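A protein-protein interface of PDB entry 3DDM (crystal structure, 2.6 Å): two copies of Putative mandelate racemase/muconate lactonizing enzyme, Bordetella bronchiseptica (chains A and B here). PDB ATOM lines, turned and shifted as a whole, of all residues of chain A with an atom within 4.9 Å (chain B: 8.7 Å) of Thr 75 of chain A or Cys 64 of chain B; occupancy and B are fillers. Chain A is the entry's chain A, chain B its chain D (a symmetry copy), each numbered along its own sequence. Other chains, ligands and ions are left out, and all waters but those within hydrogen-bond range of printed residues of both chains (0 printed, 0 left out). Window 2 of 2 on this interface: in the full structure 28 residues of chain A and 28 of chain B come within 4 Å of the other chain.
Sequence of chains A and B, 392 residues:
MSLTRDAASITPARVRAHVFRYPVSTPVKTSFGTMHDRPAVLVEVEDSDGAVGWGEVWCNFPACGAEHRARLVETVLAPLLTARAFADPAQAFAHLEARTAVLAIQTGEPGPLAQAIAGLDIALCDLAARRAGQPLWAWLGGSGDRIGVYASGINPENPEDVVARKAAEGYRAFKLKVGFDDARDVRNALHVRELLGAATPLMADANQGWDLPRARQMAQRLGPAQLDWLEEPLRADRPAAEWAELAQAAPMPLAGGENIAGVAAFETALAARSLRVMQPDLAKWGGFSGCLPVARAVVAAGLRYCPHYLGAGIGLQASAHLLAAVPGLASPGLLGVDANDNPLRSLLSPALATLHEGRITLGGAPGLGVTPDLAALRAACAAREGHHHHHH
The side-chain hydroxyl of Thr 75 of chain A lies within hydrogen-bond range of the side-chain sulfur of Cys 64 of chain B, 3.6 Å away.
Printed residues of chain B within 4 Å of His 68 of chain A: Pro 62, Cys 64, Gly 65 and His 68.
Of the printed residues of chain B, Arg 71 of chain A touches Cys 64 (3.6 Å).
Of chain B, only Cys 64 comes within 4 Å of Thr 75 of chain A.
Val 19 of chain B touches none of the printed residues of chain A.
Of the printed residues of chain A, Pro 62 of chain B touches His 68 (3.9 Å) and Leu 72 (3.8 Å).
Cys 64 of chain B touches just these residues of chain A: His 68 (3.9 Å), Arg 71 (3.6 Å) and Thr 75 (3.6 Å).
Of the printed residues of chain A, Gly 65 of chain B touches His 68 (3.5 Å).
Arg 69 of chain B touches none of the printed residues of chain A.
Printed residues of chain B that touch a printed residue of chain A: Pro 62, Cys 64, Gly 65 and His 68.
Of the 9 printed residues of chain A, 4 touch a printed residue of chain B.
The side-chain hydroxyl of Thr 75 of chain A lies within hydrogen-bond range of the backbone carbonyl oxygen of Arg 71 of chain A, at 2.9 Å.
The backbone NH (N) of Leu 77 of chain A is in hydrogen-bond range of the backbone carbonyl oxygen (O) of Leu 72 of chain A (3.1 Å).
O of Gly 65 of chain B lies within hydrogen-bond range of NH1 of Arg 69 of chain B (3.3 Å).
Among the printed residues, pairs that only touch across the chains: His 68 of chain A with Gly 65 of chain B (3.5 Å), His 68 of chain A with His 68 of chain B (3.5 Å), Arg 71 of chain A with Cys 64 of chain B (3.6 Å), Leu 72 of chain A with Pro 62 of chain B (3.8 Å), His 68 of chain A with Pro 62 of chain B (3.9 Å) and His 68 of chain A with Cys 64 of chain B (3.9 Å).
His 68 of chain B touches its own counterpart, His 68 of chain A.
1 position is printed for both chains.
Of the 7 pairs that touch across the chains among the printed residues, 1 has its exchanged pair printed and touching as well.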
ATOM      1  N   HIS A  68      11.807  33.783 -11.715  1.00  0.00           N
ATOM      2  CA  HIS A  68      11.008  32.615 -11.391  1.00  0.00           C
ATOM      3  C   HIS A  68      10.456  31.959 -12.658  1.00  0.00           C
ATOM      4  O   HIS A  68      10.450  30.733 -12.795  1.00  0.00           O
ATOM      5  CB  HIS A  68       9.848  33.016 -10.472  1.00  0.00           C
ATOM      6  CG  HIS A  68       8.983  31.868 -10.063  1.00  0.00           C
ATOM      7  ND1 HIS A  68       9.475  30.773  -9.382  1.00  0.00           N
ATOM      8  CD2 HIS A  68       7.667  31.626 -10.267  1.00  0.00           C
ATOM      9  CE1 HIS A  68       8.498  29.904  -9.187  1.00  0.00           C
ATOM     10  NE2 HIS A  68       7.391  30.398  -9.715  1.00  0.00           N
ATOM     11  N   ARG A  71      13.085  30.180 -14.534  1.00  0.00           N
ATOM     12  CA  ARG A  71      13.389  28.940 -13.825  1.00  0.00           C
ATOM     13  C   ARG A  71      12.338  27.888 -14.153  1.00  0.00           C
ATOM     14  O   ARG A  71      12.671  26.731 -14.410  1.00  0.00           O
ATOM     15  CB  ARG A  71      13.428  29.151 -12.307  1.00  0.00           C
ATOM     16  CG  ARG A  71      14.674  29.851 -11.789  1.00  0.00           C
ATOM     17  CD  ARG A  71      15.951  29.090 -12.177  1.00  0.00           C
ATOM     18  NE  ARG A  71      16.249  27.924 -11.329  1.00  0.00           N
ATOM     19  CZ  ARG A  71      17.144  26.979 -11.634  1.00  0.00           C
ATOM     20  NH1 ARG A  71      17.835  27.045 -12.772  1.00  0.00           N
ATOM     21  NH2 ARG A  71      17.358  25.971 -10.795  1.00  0.00           N
ATOM     22  N   LEU A  72      11.068  28.287 -14.142  1.00  0.00           N
ATOM     23  CA  LEU A  72       9.989  27.354 -14.455  1.00  0.00           C
ATOM     24  C   LEU A  72      10.205  26.706 -15.812  1.00  0.00           C
ATOM     25  O   LEU A  72      10.016  25.492 -15.966  1.00  0.00           O
ATOM     26  CB  LEU A  72       8.630  28.063 -14.454  1.00  0.00           C
ATOM     27  CG  LEU A  72       7.991  28.315 -13.084  1.00  0.00           C
ATOM     28  CD1 LEU A  72       6.637  28.973 -13.273  1.00  0.00           C
ATOM     29  CD2 LEU A  72       7.847  27.004 -12.331  1.00  0.00           C
ATOM     30  N   VAL A  73      10.599  27.519 -16.792  1.00  0.00           N
ATOM     31  CA  VAL A  73      10.835  27.028 -18.144  1.00  0.00           C
ATOM     32  C   VAL A  73      11.962  25.999 -18.194  1.00  0.00           C
ATOM     33  O   VAL A  73      11.826  24.953 -18.832  1.00  0.00           O
ATOM     34  CB  VAL A  73      11.164  28.191 -19.110  1.00  0.00           C
ATOM     35  CG1 VAL A  73      11.671  27.651 -20.449  1.00  0.00           C
ATOM     36  CG2 VAL A  73       9.929  29.031 -19.327  1.00  0.00           C
ATOM     37  N   GLU A  74      13.064  26.286 -17.510  1.00  0.00           N
ATOM     38  CA  GLU A  74      14.202  25.374 -17.511  1.00  0.00           C
ATOM     39  C   GLU A  74      14.090  24.177 -16.555  1.00  0.00           C
ATOM     40  O   GLU A  74      14.551  23.089 -16.881  1.00  0.00           O
ATOM     41  CB  GLU A  74      15.499  26.152 -17.235  1.00  0.00           C
ATOM     42  CG  GLU A  74      15.804  27.226 -18.287  1.00  0.00           C
ATOM     43  CD  GLU A  74      17.143  27.945 -18.075  1.00  0.00           C
ATOM     44  OE1 GLU A  74      17.418  28.388 -16.934  1.00  0.00           O
ATOM     45  OE2 GLU A  74      17.914  28.084 -19.056  1.00  0.00           O
ATOM     46  N   THR A  75      13.467  24.351 -15.393  1.00  0.00           N
ATOM     47  CA  THR A  75      13.360  23.242 -14.442  1.00  0.00           C
ATOM     48  C   THR A  75      12.081  22.405 -14.500  1.00  0.00           C
ATOM     49  O   THR A  75      12.072  21.271 -14.033  1.00  0.00           O
ATOM     50  CB  THR A  75      13.522  23.725 -12.977  1.00  0.00           C
ATOM     51  OG1 THR A  75      12.379  24.495 -12.595  1.00  0.00           O
ATOM     52  CG2 THR A  75      14.767  24.588 -12.829  1.00  0.00           C
ATOM     53  N   VAL A  76      11.008  22.938 -15.071  1.00  0.00           N
ATOM     54  CA  VAL A  76       9.756  22.191 -15.122  1.00  0.00           C
ATOM     55  C   VAL A  76       9.229  21.865 -16.514  1.00  0.00           C
ATOM     56  O   VAL A  76       8.876  20.719 -16.799  1.00  0.00           O
ATOM     57  CB  VAL A  76       8.662  22.939 -14.338  1.00  0.00           C
ATOM     58  CG1 VAL A  76       7.287  22.355 -14.637  1.00  0.00           C
ATOM     59  CG2 VAL A  76       8.971  22.866 -12.857  1.00  0.00           C
ATOM     60  N   LEU A  77       9.167  22.865 -17.383  1.00  0.00           N
ATOM     61  CA  LEU A  77       8.655  22.650 -18.728  1.00  0.00           C
ATOM     62  C   LEU A  77       9.673  22.038 -19.684  1.00  0.00           C
ATOM     63  O   LEU A  77       9.306  21.244 -20.541  1.00  0.00           O
ATOM     64  CB  LEU A  77       8.156  23.971 -19.303  1.00  0.00           C
ATOM     65  CG  LEU A  77       7.128  24.722 -18.461  1.00  0.00           C
ATOM     66  CD1 LEU A  77       7.017  26.135 -18.984  1.00  0.00           C
ATOM     67  CD2 LEU A  77       5.789  24.014 -18.500  1.00  0.00           C
ATOM     68  N   PRO A  79      12.119  19.722 -19.269  1.00  0.00           N
ATOM     69  CA  PRO A  79      12.164  18.258 -19.159  1.00  0.00           C
ATOM     70  C   PRO A  79      10.964  17.591 -19.824  1.00  0.00           C
ATOM     71  O   PRO A  79      11.112  16.593 -20.534  1.00  0.00           O
ATOM     72  CB  PRO A  79      12.183  18.023 -17.658  1.00  0.00           C
ATOM     73  CG  PRO A  79      12.909  19.237 -17.140  1.00  0.00           C
ATOM     74  CD  PRO A  79      12.283  20.349 -17.943  1.00  0.00           C
ATOM     75  N   VAL B  19      16.258  32.545   2.457  1.00  0.00           N
ATOM     76  CA  VAL B  19      16.057  31.270   1.770  1.00  0.00           C
ATOM     77  C   VAL B  19      17.106  30.257   2.172  1.00  0.00           C
ATOM     78  O   VAL B  19      18.286  30.582   2.232  1.00  0.00           O
ATOM     79  CB  VAL B  19      16.140  31.427   0.233  1.00  0.00           C
ATOM     80  CG1 VAL B  19      15.943  30.069  -0.439  1.00  0.00           C
ATOM     81  CG2 VAL B  19      15.103  32.427  -0.253  1.00  0.00           C
ATOM     82  N   ARG B  21      18.354  25.989   1.686  1.00  0.00           N
ATOM     83  CA  ARG B  21      18.173  24.776   0.909  1.00  0.00           C
ATOM     84  C   ARG B  21      19.116  23.688   1.389  1.00  0.00           C
ATOM     85  O   ARG B  21      20.325  23.763   1.183  1.00  0.00           O
ATOM     86  CB  ARG B  21      18.406  25.051  -0.578  1.00  0.00           C
ATOM     87  CG  ARG B  21      17.711  26.310  -1.071  1.00  0.00           C
ATOM     88  CD  ARG B  21      17.683  26.398  -2.582  1.00  0.00           C
ATOM     89  NE  ARG B  21      16.701  25.471  -3.127  1.00  0.00           N
ATOM     90  CZ  ARG B  21      15.672  25.843  -3.882  1.00  0.00           C
ATOM     91  NH1 ARG B  21      15.498  27.124  -4.183  1.00  0.00           N
ATOM     92  NH2 ARG B  21      14.815  24.937  -4.323  1.00  0.00           N
ATOM     93  N   ASP B  37      16.599  19.015  -2.944  1.00  0.00           N
ATOM     94  CA  ASP B  37      16.844  19.483  -1.586  1.00  0.00           C
ATOM     95  C   ASP B  37      15.550  19.900  -0.908  1.00  0.00           C
ATOM     96  O   ASP B  37      14.490  19.890  -1.526  1.00  0.00           O
ATOM     97  CB  ASP B  37      17.805  20.670  -1.613  1.00  0.00           C
ATOM     98  CG  ASP B  37      17.496  21.640  -2.734  1.00  0.00           C
ATOM     99  OD1 ASP B  37      16.329  22.073  -2.859  1.00  0.00           O
ATOM    100  OD2 ASP B  37      18.425  21.975  -3.493  1.00  0.00           O
ATOM    101  N   PRO B  39      13.775  22.978   0.575  1.00  0.00           N
ATOM    102  CA  PRO B  39      13.864  24.438   0.644  1.00  0.00           C
ATOM    103  C   PRO B  39      13.073  25.011   1.804  1.00  0.00           C
ATOM    104  O   PRO B  39      12.190  24.360   2.353  1.00  0.00           O
ATOM    105  CB  PRO B  39      13.285  24.869  -0.689  1.00  0.00           C
ATOM    106  CG  PRO B  39      12.145  23.911  -0.822  1.00  0.00           C
ATOM    107  CD  PRO B  39      12.750  22.569  -0.401  1.00  0.00           C
ATOM    108  N   VAL B  41      11.754  29.130   3.443  1.00  0.00           N
ATOM    109  CA  VAL B  41      11.735  30.581   3.360  1.00  0.00           C
ATOM    110  C   VAL B  41      11.313  31.102   4.723  1.00  0.00           C
ATOM    111  O   VAL B  41      10.151  30.973   5.106  1.00  0.00           O
ATOM    112  CB  VAL B  41      10.722  31.103   2.332  1.00  0.00           C
ATOM    113  CG1 VAL B  41      10.762  32.620   2.313  1.00  0.00           C
ATOM    114  CG2 VAL B  41      11.030  30.550   0.956  1.00  0.00           C
ATOM    115  N   CYS B  59       6.826  26.678   0.610  1.00  0.00           N
ATOM    116  CA  CYS B  59       7.516  26.726  -0.667  1.00  0.00           C
ATOM    117  C   CYS B  59       8.071  25.383  -1.127  1.00  0.00           C
ATOM    118  O   CYS B  59       9.120  25.335  -1.760  1.00  0.00           O
ATOM    119  CB  CYS B  59       8.657  27.744  -0.606  1.00  0.00           C
ATOM    120  SG  CYS B  59      10.046  27.252   0.446  1.00  0.00           S
ATOM    121  N   ASN B  60       7.378  24.291  -0.830  1.00  0.00           N
ATOM    122  CA  ASN B  60       7.869  22.984  -1.255  1.00  0.00           C
ATOM    123  C   ASN B  60       7.833  22.804  -2.774  1.00  0.00           C
ATOM    124  O   ASN B  60       8.621  22.040  -3.337  1.00  0.00           O
ATOM    125  CB  ASN B  60       7.075  21.860  -0.580  1.00  0.00           C
ATOM    126  CG  ASN B  60       7.433  21.700   0.884  1.00  0.00           C
ATOM    127  OD1 ASN B  60       8.615  21.744   1.254  1.00  0.00           O
ATOM    128  ND2 ASN B  60       6.420  21.507   1.726  1.00  0.00           N
ATOM    129  N   PHE B  61       6.917  23.513  -3.429  1.00  0.00           N
ATOM    130  CA  PHE B  61       6.778  23.436  -4.876  1.00  0.00           C
ATOM    131  C   PHE B  61       6.469  24.813  -5.472  1.00  0.00           C
ATOM    132  O   PHE B  61       5.814  25.645  -4.839  1.00  0.00           O
ATOM    133  CB  PHE B  61       5.661  22.457  -5.266  1.00  0.00           C
ATOM    134  CG  PHE B  61       5.809  21.081  -4.671  1.00  0.00           C
ATOM    135  CD1 PHE B  61       5.370  20.814  -3.370  1.00  0.00           C
ATOM    136  CD2 PHE B  61       6.395  20.046  -5.407  1.00  0.00           C
ATOM    137  CE1 PHE B  61       5.511  19.537  -2.809  1.00  0.00           C
ATOM    138  CE2 PHE B  61       6.542  18.763  -4.856  1.00  0.00           C
ATOM    139  CZ  PHE B  61       6.098  18.511  -3.552  1.00  0.00           C
ATOM    140  N   PRO B  62       6.980  25.081  -6.686  1.00  0.00           N
ATOM    141  CA  PRO B  62       7.804  24.103  -7.403  1.00  0.00           C
ATOM    142  C   PRO B  62       9.164  24.070  -6.710  1.00  0.00           C
ATOM    143  O   PRO B  62       9.344  24.709  -5.670  1.00  0.00           O
ATOM    144  CB  PRO B  62       7.856  24.672  -8.819  1.00  0.00           C
ATOM    145  CG  PRO B  62       7.816  26.145  -8.584  1.00  0.00           C
ATOM    146  CD  PRO B  62       6.769  26.294  -7.499  1.00  0.00           C
ATOM    147  N   ALA B  63      10.120  23.336  -7.262  1.00  0.00           N
ATOM    148  CA  ALA B  63      11.428  23.265  -6.628  1.00  0.00           C
ATOM    149  C   ALA B  63      12.155  24.617  -6.620  1.00  0.00           C
ATOM    150  O   ALA B  63      12.945  24.893  -5.714  1.00  0.00           O
ATOM    151  CB  ALA B  63      12.274  22.218  -7.317  1.00  0.00           C
ATOM    152  N   CYS B  64      11.865  25.467  -7.603  1.00  0.00           N
ATOM    153  CA  CYS B  64      12.524  26.768  -7.720  1.00  0.00           C
ATOM    154  C   CYS B  64      11.755  27.968  -7.164  1.00  0.00           C
ATOM    155  O   CYS B  64      12.234  29.109  -7.233  1.00  0.00           O
ATOM    156  CB  CYS B  64      12.839  27.033  -9.190  1.00  0.00           C
ATOM    157  SG  CYS B  64      11.364  27.022 -10.259  1.00  0.00           S
ATOM    158  N   GLY B  65      10.573  27.726  -6.609  1.00  0.00           N
ATOM    159  CA  GLY B  65       9.771  28.828  -6.092  1.00  0.00           C
ATOM    160  C   GLY B  65      10.189  29.554  -4.819  1.00  0.00           C
ATOM    161  O   GLY B  65       9.623  30.608  -4.503  1.00  0.00           O
ATOM    162  N   ALA B  66      11.170  29.019  -4.094  1.00  0.00           N
ATOM    163  CA  ALA B  66      11.609  29.627  -2.846  1.00  0.00           C
ATOM    164  C   ALA B  66      12.117  31.052  -3.023  1.00  0.00           C
ATOM    165  O   ALA B  66      11.697  31.964  -2.310  1.00  0.00           O
ATOM    166  CB  ALA B  66      12.672  28.767  -2.201  1.00  0.00           C
ATOM    167  N   GLU B  67      13.023  31.251  -3.970  1.00  0.00           N
ATOM    168  CA  GLU B  67      13.575  32.578  -4.212  1.00  0.00           C
ATOM    169  C   GLU B  67      12.488  33.592  -4.582  1.00  0.00           C
ATOM    170  O   GLU B  67      12.492  34.727  -4.099  1.00  0.00           O
ATOM    171  CB  GLU B  67      14.632  32.525  -5.325  1.00  0.00           C
ATOM    172  CG  GLU B  67      15.918  31.787  -4.973  1.00  0.00           C
ATOM    173  CD  GLU B  67      15.733  30.281  -4.769  1.00  0.00           C
ATOM    174  OE1 GLU B  67      14.856  29.670  -5.432  1.00  0.00           O
ATOM    175  OE2 GLU B  67      16.491  29.697  -3.956  1.00  0.00           O
ATOM    176  N   HIS B  68      11.562  33.182  -5.442  1.00  0.00           N
ATOM    177  CA  HIS B  68      10.488  34.070  -5.869  1.00  0.00           C
ATOM    178  C   HIS B  68       9.632  34.515  -4.686  1.00  0.00           C
ATOM    179  O   HIS B  68       9.340  35.701  -4.538  1.00  0.00           O
ATOM    180  CB  HIS B  68       9.616  33.379  -6.925  1.00  0.00           C
ATOM    181  CG  HIS B  68       8.484  34.224  -7.414  1.00  0.00           C
ATOM    182  ND1 HIS B  68       8.661  35.508  -7.881  1.00  0.00           N
ATOM    183  CD2 HIS B  68       7.152  33.986  -7.472  1.00  0.00           C
ATOM    184  CE1 HIS B  68       7.490  36.027  -8.200  1.00  0.00           C
ATOM    185  NE2 HIS B  68       6.558  35.124  -7.961  1.00  0.00           N
ATOM    186  N   ARG B  69       9.232  33.568  -3.843  1.00  0.00           N
ATOM    187  CA  ARG B  69       8.419  33.889  -2.678  1.00  0.00           C
ATOM    188  C   ARG B  69       9.140  34.866  -1.750  1.00  0.00           C
ATOM    189  O   ARG B  69       8.533  35.807  -1.227  1.00  0.00           O
ATOM    190  CB  ARG B  69       8.026  32.595  -1.953  1.00  0.00           C
ATOM    191  CG  ARG B  69       6.897  31.862  -2.685  1.00  0.00           C
ATOM    192  CD  ARG B  69       6.903  30.353  -2.489  1.00  0.00           C
ATOM    193  NE  ARG B  69       5.730  29.735  -3.106  1.00  0.00           N
ATOM    194  CZ  ARG B  69       5.558  29.563  -4.416  1.00  0.00           C
ATOM    195  NH1 ARG B  69       6.493  29.947  -5.282  1.00  0.00           N
ATOM    196  NH2 ARG B  69       4.424  29.039  -4.869  1.00  0.00           N
ATOM    197  N   ALA B  70      10.437  34.660  -1.555  1.00  0.00           N
ATOM    198  CA  ALA B  70      11.213  35.556  -0.707  1.00  0.00           C
ATOM    199  C   ALA B  70      11.304  36.955  -1.345  1.00  0.00           C
ATOM    200  O   ALA B  70      11.333  37.972  -0.641  1.00  0.00           O
ATOM    201  CB  ALA B  70      12.609  34.978  -0.482  1.00  0.00           C
